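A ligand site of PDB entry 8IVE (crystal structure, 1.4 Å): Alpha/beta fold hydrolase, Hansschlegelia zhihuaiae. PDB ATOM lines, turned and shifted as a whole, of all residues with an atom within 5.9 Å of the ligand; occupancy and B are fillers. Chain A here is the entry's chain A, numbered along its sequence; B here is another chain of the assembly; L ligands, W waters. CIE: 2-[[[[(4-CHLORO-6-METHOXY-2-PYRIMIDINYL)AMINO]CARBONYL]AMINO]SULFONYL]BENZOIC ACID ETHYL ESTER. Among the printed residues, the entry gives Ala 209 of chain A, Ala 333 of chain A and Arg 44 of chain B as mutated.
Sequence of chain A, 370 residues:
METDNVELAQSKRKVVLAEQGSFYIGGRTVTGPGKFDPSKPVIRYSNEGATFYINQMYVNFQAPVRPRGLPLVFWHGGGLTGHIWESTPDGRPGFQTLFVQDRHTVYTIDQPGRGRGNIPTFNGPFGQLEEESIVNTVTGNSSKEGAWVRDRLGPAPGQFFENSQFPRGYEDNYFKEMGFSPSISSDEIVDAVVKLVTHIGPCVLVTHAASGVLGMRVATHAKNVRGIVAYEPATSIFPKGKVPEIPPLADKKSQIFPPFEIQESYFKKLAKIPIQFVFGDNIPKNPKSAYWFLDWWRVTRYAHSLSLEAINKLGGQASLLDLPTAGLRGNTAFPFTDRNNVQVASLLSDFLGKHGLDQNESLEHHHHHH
The backbone carbonyl oxygen (O) of Arg 150 sits at hydrogen-bond distance from the indole nitrogen (NE1) of Trp 297. The backbone NH (N) of Gly 146 sits at hydrogen-bond distance from the side-chain hydroxyl (OG) of Ser 143 (3.0 Å). N of Ala 234 sits at hydrogen-bond distance from O of Ala 209, at 3.0 Å. The backbone carbonyl oxygen of Glu 232 lies close to the backbone NH of Ala 209. The side-chain amide nitrogen of Asn 123 of chain B is in hydrogen-bond range of the backbone carbonyl oxygen of Ser 46 of chain B (3.1 Å). The backbone carbonyl oxygen of Asp 151 lies within hydrogen-bond range of the backbone NH of Ala 333 (3.0 Å). The backbone NH (N) of His 208 is in hydrogen-bond range of the side-chain hydroxyl (OG) of Ser 211 (2.9 Å). A ring nitrogen (NE2) of His 208 sits at hydrogen-bond distance from the backbone carbonyl oxygen (O) of Ala 333, at 3.0 Å.
N of Gly 78 is in hydrogen-bond range of O7 of the ligand, 2.8 Å away. An oxygen (O13) of the ligand sits at hydrogen-bond distance from the guanidinium group (NH1) of Arg 150. N of Ala 210 lies within hydrogen-bond range of O7 of the ligand, at 3.1 Å.
O of Asn 141 sits close to O7' of the ligand, at 3.5 Å. Residues that only touch the ligand: Gly 146, Ala 209, Phe 334, Arg 44 of chain B, Ala 147, Val 42 of chain B, Phe 257, Trp 296, Asn 123 of chain B, Phe 293, Ser 142, Asp 151, His 208, Ala 234, Gly 77, Leu 80 and Ile 43 of chain B. Hydrophobic or aromatic side chains within 4 Å of the ligand: Leu 80, His 208, Ala 209, Ala 210, Ala 234, Phe 257, Phe 293, Trp 296, Phe 334, Val 42 of chain B and Ile 43 of chain B. Of the 32 residues printed, 21 come within 4 Å of the ligand.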
ATOM      1  N   GLY A  77       8.132  31.579  -2.026  1.00  0.00           N
ATOM      2  CA  GLY A  77       7.219  30.493  -2.315  1.00  0.00           C
ATOM      3  C   GLY A  77       7.141  30.164  -3.796  1.00  0.00           C
ATOM      4  O   GLY A  77       7.953  30.587  -4.620  1.00  0.00           O
ATOM      5  N   GLY A  78       6.111  29.390  -4.135  1.00  0.00           N
ATOM      6  CA  GLY A  78       6.020  28.789  -5.454  1.00  0.00           C
ATOM      7  C   GLY A  78       5.814  29.832  -6.526  1.00  0.00           C
ATOM      8  O   GLY A  78       4.936  30.700  -6.404  1.00  0.00           O
ATOM      9  N   GLY A  79       6.628  29.766  -7.585  1.00  0.00           N
ATOM     10  CA  GLY A  79       6.484  30.670  -8.699  1.00  0.00           C
ATOM     11  C   GLY A  79       6.982  32.074  -8.457  1.00  0.00           C
ATOM     12  O   GLY A  79       6.666  32.979  -9.242  1.00  0.00           O
ATOM     13  N   LEU A  80       7.774  32.286  -7.424  1.00  0.00           N
ATOM     14  CA  LEU A  80       8.187  33.616  -6.995  1.00  0.00           C
ATOM     15  C   LEU A  80       9.701  33.748  -7.060  1.00  0.00           C
ATOM     16  O   LEU A  80      10.407  32.846  -7.547  1.00  0.00           O
ATOM     17  CB  LEU A  80       7.652  33.903  -5.593  1.00  0.00           C
ATOM     18  CG  LEU A  80       6.132  33.806  -5.454  1.00  0.00           C
ATOM     19  CD1 LEU A  80       5.773  33.698  -4.020  1.00  0.00           C
ATOM     20  CD2 LEU A  80       5.505  35.024  -6.092  1.00  0.00           C
ATOM     21  N   GLY A 140       3.361  24.124 -16.633  1.00  0.00           N
ATOM     22  CA  GLY A 140       2.163  24.597 -15.992  1.00  0.00           C
ATOM     23  C   GLY A 140       2.408  25.963 -15.383  1.00  0.00           C
ATOM     24  O   GLY A 140       3.540  26.381 -15.178  1.00  0.00           O
ATOM     25  N   ASN A 141       1.312  26.677 -15.116  1.00  0.00           N
ATOM     26  CA  ASN A 141       1.457  28.011 -14.552  1.00  0.00           C
ATOM     27  C   ASN A 141       0.147  28.434 -13.906  1.00  0.00           C
ATOM     28  O   ASN A 141      -0.928  27.985 -14.304  1.00  0.00           O
ATOM     29  CB  ASN A 141       1.847  29.040 -15.631  1.00  0.00           C
ATOM     30  CG  ASN A 141       2.631  30.215 -15.072  1.00  0.00           C
ATOM     31  OD1 ASN A 141       2.777  30.374 -13.857  1.00  0.00           O
ATOM     32  ND2 ASN A 141       3.137  31.053 -15.960  1.00  0.00           N
ATOM     33  N   SER A 142       0.262  29.307 -12.914  1.00  0.00           N
ATOM     34  CA  SER A 142      -0.889  29.937 -12.308  1.00  0.00           C
ATOM     35  C   SER A 142      -1.388  31.042 -13.225  1.00  0.00           C
ATOM     36  O   SER A 142      -0.692  31.502 -14.118  1.00  0.00           O
ATOM     37  CB  SER A 142      -0.512  30.537 -10.948  1.00  0.00           C
ATOM     38  OG  SER A 142       0.471  31.557 -11.092  1.00  0.00           O
ATOM     39  N   SER A 143      -2.633  31.451 -12.995  1.00  0.00           N
ATOM     40  CA  SER A 143      -3.224  32.605 -13.640  1.00  0.00           C
ATOM     41  C   SER A 143      -3.480  33.668 -12.592  1.00  0.00           C
ATOM     42  O   SER A 143      -3.378  33.426 -11.388  1.00  0.00           O
ATOM     43  CB  SER A 143      -4.548  32.212 -14.311  1.00  0.00           C
ATOM     44  OG  SER A 143      -5.548  31.959 -13.340  1.00  0.00           O
ATOM     45  N   GLU A 145      -6.366  34.808 -11.916  1.00  0.00           N
ATOM     46  CA  GLU A 145      -7.571  34.394 -11.211  1.00  0.00           C
ATOM     47  C   GLU A 145      -7.272  33.323 -10.167  1.00  0.00           C
ATOM     48  O   GLU A 145      -7.774  33.386  -9.035  1.00  0.00           O
ATOM     49  CB  GLU A 145      -8.587  33.866 -12.227  1.00  0.00           C
ATOM     50  CG  GLU A 145      -9.210  34.960 -13.121  1.00  0.00           C
ATOM     51  CD  GLU A 145      -8.330  35.423 -14.281  1.00  0.00           C
ATOM     52  OE1 GLU A 145      -7.202  34.898 -14.486  1.00  0.00           O
ATOM     53  OE2 GLU A 145      -8.766  36.339 -15.006  1.00  0.00           O
ATOM     54  N   GLY A 146      -6.465  32.336 -10.535  1.00  0.00           N
ATOM     55  CA  GLY A 146      -6.113  31.307  -9.574  1.00  0.00           C
ATOM     56  C   GLY A 146      -5.268  31.833  -8.429  1.00  0.00           C
ATOM     57  O   GLY A 146      -5.445  31.423  -7.280  1.00  0.00           O
ATOM     58  N   ALA A 147      -4.343  32.736  -8.741  1.00  0.00           N
ATOM     59  CA  ALA A 147      -3.495  33.297  -7.687  1.00  0.00           C
ATOM     60  C   ALA A 147      -4.314  34.169  -6.744  1.00  0.00           C
ATOM     61  O   ALA A 147      -4.052  34.196  -5.536  1.00  0.00           O
ATOM     62  CB  ALA A 147      -2.317  34.069  -8.288  1.00  0.00           C
ATOM     63  N   VAL A 149      -7.358  33.751  -5.641  1.00  0.00           N
ATOM     64  CA  VAL A 149      -8.031  32.947  -4.629  1.00  0.00           C
ATOM     65  C   VAL A 149      -7.024  32.124  -3.818  1.00  0.00           C
ATOM     66  O   VAL A 149      -7.193  31.946  -2.604  1.00  0.00           O
ATOM     67  CB  VAL A 149      -9.171  32.094  -5.229  1.00  0.00           C
ATOM     68  CG1 VAL A 149     -10.287  33.036  -5.736  1.00  0.00           C
ATOM     69  CG2 VAL A 149      -8.671  31.197  -6.359  1.00  0.00           C
ATOM     70  N   ARG A 150      -5.964  31.645  -4.462  1.00  0.00           N
ATOM     71  CA  ARG A 150      -4.886  30.959  -3.754  1.00  0.00           C
ATOM     72  C   ARG A 150      -4.331  31.823  -2.628  1.00  0.00           C
ATOM     73  O   ARG A 150      -4.075  31.351  -1.525  1.00  0.00           O
ATOM     74  CB  ARG A 150      -3.767  30.641  -4.735  1.00  0.00           C
ATOM     75  CG  ARG A 150      -2.570  29.929  -4.115  1.00  0.00           C
ATOM     76  CD  ARG A 150      -1.378  29.961  -5.041  1.00  0.00           C
ATOM     77  NE  ARG A 150      -0.815  31.311  -5.166  1.00  0.00           N
ATOM     78  CZ  ARG A 150       0.091  31.673  -6.063  1.00  0.00           C
ATOM     79  NH1 ARG A 150       0.542  30.787  -6.958  1.00  0.00           N
ATOM     80  NH2 ARG A 150       0.552  32.917  -6.079  1.00  0.00           N
ATOM     81  N   ASP A 151      -4.131  33.114  -2.900  1.00  0.00           N
ATOM     82  CA  ASP A 151      -3.498  33.978  -1.920  1.00  0.00           C
ATOM     83  C   ASP A 151      -4.497  34.606  -0.963  1.00  0.00           C
ATOM     84  O   ASP A 151      -4.103  35.338  -0.050  1.00  0.00           O
ATOM     85  CB  ASP A 151      -2.616  35.010  -2.628  1.00  0.00           C
ATOM     86  CG  ASP A 151      -1.516  34.345  -3.464  1.00  0.00           C
ATOM     87  OD1 ASP A 151      -1.202  33.181  -3.147  1.00  0.00           O
ATOM     88  OD2 ASP A 151      -0.963  34.965  -4.403  1.00  0.00           O
ATOM     89  N   HIS A 208       8.138  30.087   2.758  1.00  0.00           N
ATOM     90  CA  HIS A 208       6.855  30.609   2.313  1.00  0.00           C
ATOM     91  C   HIS A 208       6.205  29.591   1.407  1.00  0.00           C
ATOM     92  O   HIS A 208       6.796  29.176   0.406  1.00  0.00           O
ATOM     93  CB  HIS A 208       7.083  31.908   1.537  1.00  0.00           C
ATOM     94  CG  HIS A 208       5.857  32.486   0.923  1.00  0.00           C
ATOM     95  ND1 HIS A 208       5.835  32.970  -0.368  1.00  0.00           N
ATOM     96  CD2 HIS A 208       4.620  32.685   1.422  1.00  0.00           C
ATOM     97  CE1 HIS A 208       4.631  33.435  -0.633  1.00  0.00           C
ATOM     98  NE2 HIS A 208       3.865  33.269   0.431  1.00  0.00           N
ATOM     99  N   ALA A 209       4.980  29.180   1.743  1.00  0.00           N
ATOM    100  CA  ALA A 209       4.174  28.383   0.817  1.00  0.00           C
ATOM    101  C   ALA A 209       4.938  27.163   0.302  1.00  0.00           C
ATOM    102  O   ALA A 209       5.315  26.308   1.109  1.00  0.00           O
ATOM    103  CB  ALA A 209       3.601  29.254  -0.300  1.00  0.00           C
ATOM    104  N   ALA A 210       5.195  27.087  -1.012  1.00  0.00           N
ATOM    105  CA  ALA A 210       5.886  25.923  -1.594  1.00  0.00           C
ATOM    106  C   ALA A 210       7.249  25.649  -0.949  1.00  0.00           C
ATOM    107  O   ALA A 210       7.701  24.500  -0.942  1.00  0.00           O
ATOM    108  CB  ALA A 210       6.038  26.064  -3.100  1.00  0.00           C
ATOM    109  N   SER A 211       7.935  26.681  -0.440  1.00  0.00           N
ATOM    110  CA  SER A 211       9.252  26.403   0.132  1.00  0.00           C
ATOM    111  C   SER A 211       9.184  25.894   1.569  1.00  0.00           C
ATOM    112  O   SER A 211      10.224  25.511   2.116  1.00  0.00           O
ATOM    113  CB  SER A 211      10.223  27.601   0.012  1.00  0.00           C
ATOM    114  OG  SER A 211       9.765  28.699   0.795  1.00  0.00           O
ATOM    115  N   GLU A 232       2.607  30.350   5.808  1.00  0.00           N
ATOM    116  CA  GLU A 232       1.605  29.671   4.990  1.00  0.00           C
ATOM    117  C   GLU A 232       2.179  28.488   4.202  1.00  0.00           C
ATOM    118  O   GLU A 232       2.008  28.426   2.973  1.00  0.00           O
ATOM    119  CB  GLU A 232       0.925  30.658   4.050  1.00  0.00           C
ATOM    120  CG  GLU A 232       0.293  31.828   4.781  1.00  0.00           C
ATOM    121  CD  GLU A 232      -1.215  31.776   4.713  1.00  0.00           C
ATOM    122  OE1 GLU A 232      -1.755  31.051   3.847  1.00  0.00           O
ATOM    123  OE2 GLU A 232      -1.871  32.444   5.526  1.00  0.00           O
ATOM    124  N   ALA A 234       2.738  25.116   2.184  1.00  0.00           N
ATOM    125  CA  ALA A 234       1.780  24.515   1.257  1.00  0.00           C
ATOM    126  C   ALA A 234       1.691  22.989   1.370  1.00  0.00           C
ATOM    127  O   ALA A 234       0.631  22.433   1.043  1.00  0.00           O
ATOM    128  CB  ALA A 234       2.084  24.913  -0.187  1.00  0.00           C
ATOM    129  N   PHE A 257      -2.409  18.609  -0.864  1.00  0.00           N
ATOM    130  CA  PHE A 257      -1.195  18.036  -1.454  1.00  0.00           C
ATOM    131  C   PHE A 257      -0.804  16.807  -0.643  1.00  0.00           C
ATOM    132  O   PHE A 257      -0.809  16.874   0.595  1.00  0.00           O
ATOM    133  CB  PHE A 257      -0.067  19.063  -1.410  1.00  0.00           C
ATOM    134  CG  PHE A 257      -0.199  20.174  -2.425  1.00  0.00           C
ATOM    135  CD1 PHE A 257      -1.156  20.142  -3.421  1.00  0.00           C
ATOM    136  CD2 PHE A 257       0.654  21.275  -2.363  1.00  0.00           C
ATOM    137  CE1 PHE A 257      -1.263  21.181  -4.342  1.00  0.00           C
ATOM    138  CE2 PHE A 257       0.565  22.299  -3.265  1.00  0.00           C
ATOM    139  CZ  PHE A 257      -0.389  22.249  -4.262  1.00  0.00           C
ATOM    140  N   PHE A 293     -10.294  27.097  -2.968  1.00  0.00           N
ATOM    141  CA  PHE A 293      -8.999  27.370  -2.335  1.00  0.00           C
ATOM    142  C   PHE A 293      -9.140  27.762  -0.872  1.00  0.00           C
ATOM    143  O   PHE A 293      -8.231  27.493  -0.075  1.00  0.00           O
ATOM    144  CB  PHE A 293      -8.184  28.369  -3.164  1.00  0.00           C
ATOM    145  CG  PHE A 293      -6.757  27.963  -3.311  1.00  0.00           C
ATOM    146  CD1 PHE A 293      -6.051  27.498  -2.210  1.00  0.00           C
ATOM    147  CD2 PHE A 293      -6.135  27.975  -4.549  1.00  0.00           C
ATOM    148  CE1 PHE A 293      -4.741  27.093  -2.320  1.00  0.00           C
ATOM    149  CE2 PHE A 293      -4.802  27.551  -4.670  1.00  0.00           C
ATOM    150  CZ  PHE A 293      -4.126  27.108  -3.542  1.00  0.00           C
ATOM    151  N   TRP A 296      -9.316  24.401   0.703  1.00  0.00           N
ATOM    152  CA  TRP A 296      -7.994  23.796   0.633  1.00  0.00           C
ATOM    153  C   TRP A 296      -7.113  24.281   1.779  1.00  0.00           C
ATOM    154  O   TRP A 296      -6.431  23.482   2.435  1.00  0.00           O
ATOM    155  CB  TRP A 296      -7.372  24.133  -0.734  1.00  0.00           C
ATOM    156  CG  TRP A 296      -6.081  23.451  -1.067  1.00  0.00           C
ATOM    157  CD1 TRP A 296      -5.911  22.325  -1.821  1.00  0.00           C
ATOM    158  CD2 TRP A 296      -4.771  23.883  -0.686  1.00  0.00           C
ATOM    159  NE1 TRP A 296      -4.575  22.024  -1.938  1.00  0.00           N
ATOM    160  CE2 TRP A 296      -3.852  22.957  -1.244  1.00  0.00           C
ATOM    161  CE3 TRP A 296      -4.276  24.955   0.057  1.00  0.00           C
ATOM    162  CZ2 TRP A 296      -2.473  23.079  -1.064  1.00  0.00           C
ATOM    163  CZ3 TRP A 296      -2.909  25.075   0.233  1.00  0.00           C
ATOM    164  CH2 TRP A 296      -2.027  24.143  -0.329  1.00  0.00           C
ATOM    165  N   TRP A 297      -7.136  25.593   2.037  1.00  0.00           N
ATOM    166  CA  TRP A 297      -6.334  26.138   3.132  1.00  0.00           C
ATOM    167  C   TRP A 297      -6.833  25.641   4.483  1.00  0.00           C
ATOM    168  O   TRP A 297      -6.028  25.423   5.396  1.00  0.00           O
ATOM    169  CB  TRP A 297      -6.336  27.668   3.067  1.00  0.00           C
ATOM    170  CG  TRP A 297      -5.322  28.228   2.122  1.00  0.00           C
ATOM    171  CD1 TRP A 297      -5.554  28.970   0.998  1.00  0.00           C
ATOM    172  CD2 TRP A 297      -3.885  28.096   2.220  1.00  0.00           C
ATOM    173  NE1 TRP A 297      -4.373  29.303   0.393  1.00  0.00           N
ATOM    174  CE2 TRP A 297      -3.336  28.784   1.120  1.00  0.00           C
ATOM    175  CE3 TRP A 297      -3.027  27.470   3.131  1.00  0.00           C
ATOM    176  CZ2 TRP A 297      -1.957  28.868   0.900  1.00  0.00           C
ATOM    177  CZ3 TRP A 297      -1.648  27.537   2.895  1.00  0.00           C
ATOM    178  CH2 TRP A 297      -1.129  28.232   1.792  1.00  0.00           C
ATOM    179  N   ALA A 333      -1.947  35.392   2.018  1.00  0.00           N
ATOM    180  CA  ALA A 333      -0.914  34.363   2.096  1.00  0.00           C
ATOM    181  C   ALA A 333       0.495  34.925   1.913  1.00  0.00           C
ATOM    182  O   ALA A 333       1.454  34.140   1.919  1.00  0.00           O
ATOM    183  CB  ALA A 333      -1.191  33.284   1.046  1.00  0.00           C
ATOM    184  N   PHE A 334       0.634  36.246   1.735  1.00  0.00           N
ATOM    185  CA  PHE A 334       1.934  36.926   1.714  1.00  0.00           C
ATOM    186  C   PHE A 334       1.924  37.968   2.829  1.00  0.00           C
ATOM    187  O   PHE A 334       1.954  39.183   2.562  1.00  0.00           O
ATOM    188  CB  PHE A 334       2.169  37.679   0.401  1.00  0.00           C
ATOM    189  CG  PHE A 334       2.368  36.819  -0.838  1.00  0.00           C
ATOM    190  CD1 PHE A 334       1.493  35.808  -1.186  1.00  0.00           C
ATOM    191  CD2 PHE A 334       3.399  37.131  -1.717  1.00  0.00           C
ATOM    192  CE1 PHE A 334       1.675  35.082  -2.375  1.00  0.00           C
ATOM    193  CE2 PHE A 334       3.586  36.417  -2.906  1.00  0.00           C
ATOM    194  CZ  PHE A 334       2.710  35.400  -3.233  1.00  0.00           C
ATOM    195  N   VAL B  42      -8.717  24.484  -8.380  1.00  0.00           N
ATOM    196  CA  VAL B  42      -7.973  25.591  -8.988  1.00  0.00           C
ATOM    197  C   VAL B  42      -6.671  25.117  -9.600  1.00  0.00           C
ATOM    198  O   VAL B  42      -6.231  25.624 -10.636  1.00  0.00           O
ATOM    199  CB  VAL B  42      -7.755  26.720  -7.964  1.00  0.00           C
ATOM    200  CG1 VAL B  42      -6.868  27.823  -8.563  1.00  0.00           C
ATOM    201  CG2 VAL B  42      -9.099  27.304  -7.528  1.00  0.00           C
ATOM    202  N   ILE B  43      -6.072  24.170  -8.954  1.00  0.00           N
ATOM    203  CA  ILE B  43      -4.857  23.629  -9.486  1.00  0.00           C
ATOM    204  C   ILE B  43      -5.164  22.518 -10.491  1.00  0.00           C
ATOM    205  O   ILE B  43      -5.465  21.418 -10.083  1.00  0.00           O
ATOM    206  CB  ILE B  43      -3.954  23.150  -8.368  1.00  0.00           C
ATOM    207  CG1 ILE B  43      -3.593  24.342  -7.481  1.00  0.00           C
ATOM    208  CG2 ILE B  43      -2.670  22.552  -8.933  1.00  0.00           C
ATOM    209  CD1 ILE B  43      -3.118  23.944  -6.118  1.00  0.00           C
ATOM    210  N   ARG B  44      -5.074  22.833 -11.767  1.00  0.00           N
ATOM    211  CA  ARG B  44      -5.303  21.849 -12.799  1.00  0.00           C
ATOM    212  C   ARG B  44      -4.695  22.280 -14.110  1.00  0.00           C
ATOM    213  O   ARG B  44      -4.401  23.458 -14.292  1.00  0.00           O
ATOM    214  CB  ARG B  44      -6.796  21.523 -12.951  1.00  0.00           C
ATOM    215  CG  ARG B  44      -7.617  22.712 -13.380  1.00  0.00           C
ATOM    216  CD  ARG B  44      -9.091  22.451 -13.311  1.00  0.00           C
ATOM    217  NE  ARG B  44      -9.739  23.668 -13.718  1.00  0.00           N
ATOM    218  CZ  ARG B  44     -10.853  23.731 -14.419  1.00  0.00           C
ATOM    219  NH1 ARG B  44     -11.477  22.610 -14.754  1.00  0.00           N
ATOM    220  NH2 ARG B  44     -11.347  24.900 -14.770  1.00  0.00           N
ATOM    221  N   TYR B  45      -4.513  21.318 -15.001  1.00  0.00           N
ATOM    222  CA  TYR B  45      -3.969  21.567 -16.319  1.00  0.00           C
ATOM    223  C   TYR B  45      -5.008  22.170 -17.178  1.00  0.00           C
ATOM    224  O   TYR B  45      -5.732  21.441 -17.848  1.00  0.00           O
ATOM    225  CB  TYR B  45      -3.418  20.243 -16.881  1.00  0.00           C
ATOM    226  CG  TYR B  45      -2.621  20.242 -18.178  1.00  0.00           C
ATOM    227  CD1 TYR B  45      -2.740  21.239 -19.128  1.00  0.00           C
ATOM    228  CD2 TYR B  45      -1.757  19.199 -18.442  1.00  0.00           C
ATOM    229  CE1 TYR B  45      -2.011  21.218 -20.295  1.00  0.00           C
ATOM    230  CE2 TYR B  45      -1.022  19.167 -19.603  1.00  0.00           C
ATOM    231  CZ  TYR B  45      -1.160  20.182 -20.514  1.00  0.00           C
ATOM    232  OH  TYR B  45      -0.437  20.140 -21.659  1.00  0.00           O
ATOM    233  N   SER B  46      -5.093  23.506 -17.183  1.00  0.00           N
ATOM    234  CA  SER B  46      -6.047  24.194 -18.036  1.00  0.00           C
ATOM    235  C   SER B  46      -5.738  25.674 -18.029  1.00  0.00           C
ATOM    236  O   SER B  46      -5.242  26.219 -17.037  1.00  0.00           O
ATOM    237  CB  SER B  46      -7.493  23.959 -17.570  1.00  0.00           C
ATOM    238  OG  SER B  46      -8.385  24.768 -18.319  1.00  0.00           O
ATOM    239  N   ASN B 123      -0.123  26.676 -19.446  1.00  0.00           N
ATOM    240  CA  ASN B 123      -0.400  25.264 -19.240  1.00  0.00           C
ATOM    241  C   ASN B 123      -0.434  24.619 -20.625  1.00  0.00           C
ATOM    242  O   ASN B 123      -1.379  24.797 -21.379  1.00  0.00           O
ATOM    243  CB  ASN B 123      -1.694  25.089 -18.463  1.00  0.00           C
ATOM    244  CG  ASN B 123      -1.620  25.707 -17.091  1.00  0.00           C
ATOM    245  OD1 ASN B 123      -0.993  25.158 -16.176  1.00  0.00           O
ATOM    246  ND2 ASN B 123      -2.239  26.875 -16.933  1.00  0.00           N
HETATM  247  C1  CIE L   1       1.370  27.651  -3.421  1.00  0.00           C
HETATM  248  C2  CIE L   1       1.328  26.660  -4.377  1.00  0.00           C
HETATM  249  C3  CIE L   1       0.291  25.742  -4.236  1.00  0.00           C
HETATM  250  C4  CIE L   1      -0.642  25.826  -3.210  1.00  0.00           C
HETATM  251  C5  CIE L   1      -0.569  26.841  -2.279  1.00  0.00           C
HETATM  252  C6  CIE L   1       0.442  27.771  -2.402  1.00  0.00           C
HETATM  253  C7  CIE L   1       2.426  28.678  -3.481  1.00  0.00           C
HETATM  254  O7  CIE L   1       3.589  28.497  -3.270  1.00  0.00           O
HETATM  255  O8  CIE L   1       1.970  29.938  -3.861  1.00  0.00           O
HETATM  256  C9  CIE L   1       2.950  30.905  -4.014  1.00  0.00           C
HETATM  257  C10 CIE L   1       2.285  31.806  -3.098  1.00  0.00           C
HETATM  258  S11 CIE L   1       2.368  26.515  -5.611  1.00  0.00           S
HETATM  259  OBA CIE L   1       3.382  25.592  -5.326  1.00  0.00           O
HETATM  260  OBB CIE L   1       2.988  27.698  -6.086  1.00  0.00           O
HETATM  261  N12 CIE L   1       1.577  26.024  -6.877  1.00  0.00           N
HETATM  262  C13 CIE L   1       0.679  26.776  -7.485  1.00  0.00           C
HETATM  263  O13 CIE L   1       0.360  27.841  -7.013  1.00  0.00           O
HETATM  264  N14 CIE L   1       0.198  26.284  -8.619  1.00  0.00           N
HETATM  265  N1' CIE L   1      -1.258  26.086 -10.406  1.00  0.00           N
HETATM  266  C2' CIE L   1      -0.919  26.677  -9.263  1.00  0.00           C
HETATM  267  N3' CIE L   1      -1.699  27.631  -8.764  1.00  0.00           N
HETATM  268  C4' CIE L   1      -2.787  28.027  -9.369  1.00  0.00           C
HETATM  269 CL4' CIE L   1      -3.689  29.333  -8.561  1.00  0.00          CL
HETATM  270  C5' CIE L   1      -3.171  27.449 -10.556  1.00  0.00           C
HETATM  271  C6' CIE L   1      -2.361  26.465 -11.060  1.00  0.00           C
HETATM  272  O7' CIE L   1      -2.670  25.845 -12.208  1.00  0.00           O
HETATM  273  C8' CIE L   1      -1.748  24.865 -12.648  1.00  0.00           C
HETATM  274  O   HOH W   1       5.865  23.559  -6.621  1.00  0.00           O
HETATM  275  O   HOH W   2       1.646  24.284 -10.227  1.00  0.00           O
HETATM  276  O   HOH W   3      -5.078  29.423 -12.358  1.00  0.00           O
HETATM  277  O   HOH W   4       3.538  23.711  -3.583  1.00  0.00           O
HETATM  278  O   HOH W   5       1.597  23.184  -7.404  1.00  0.00           O
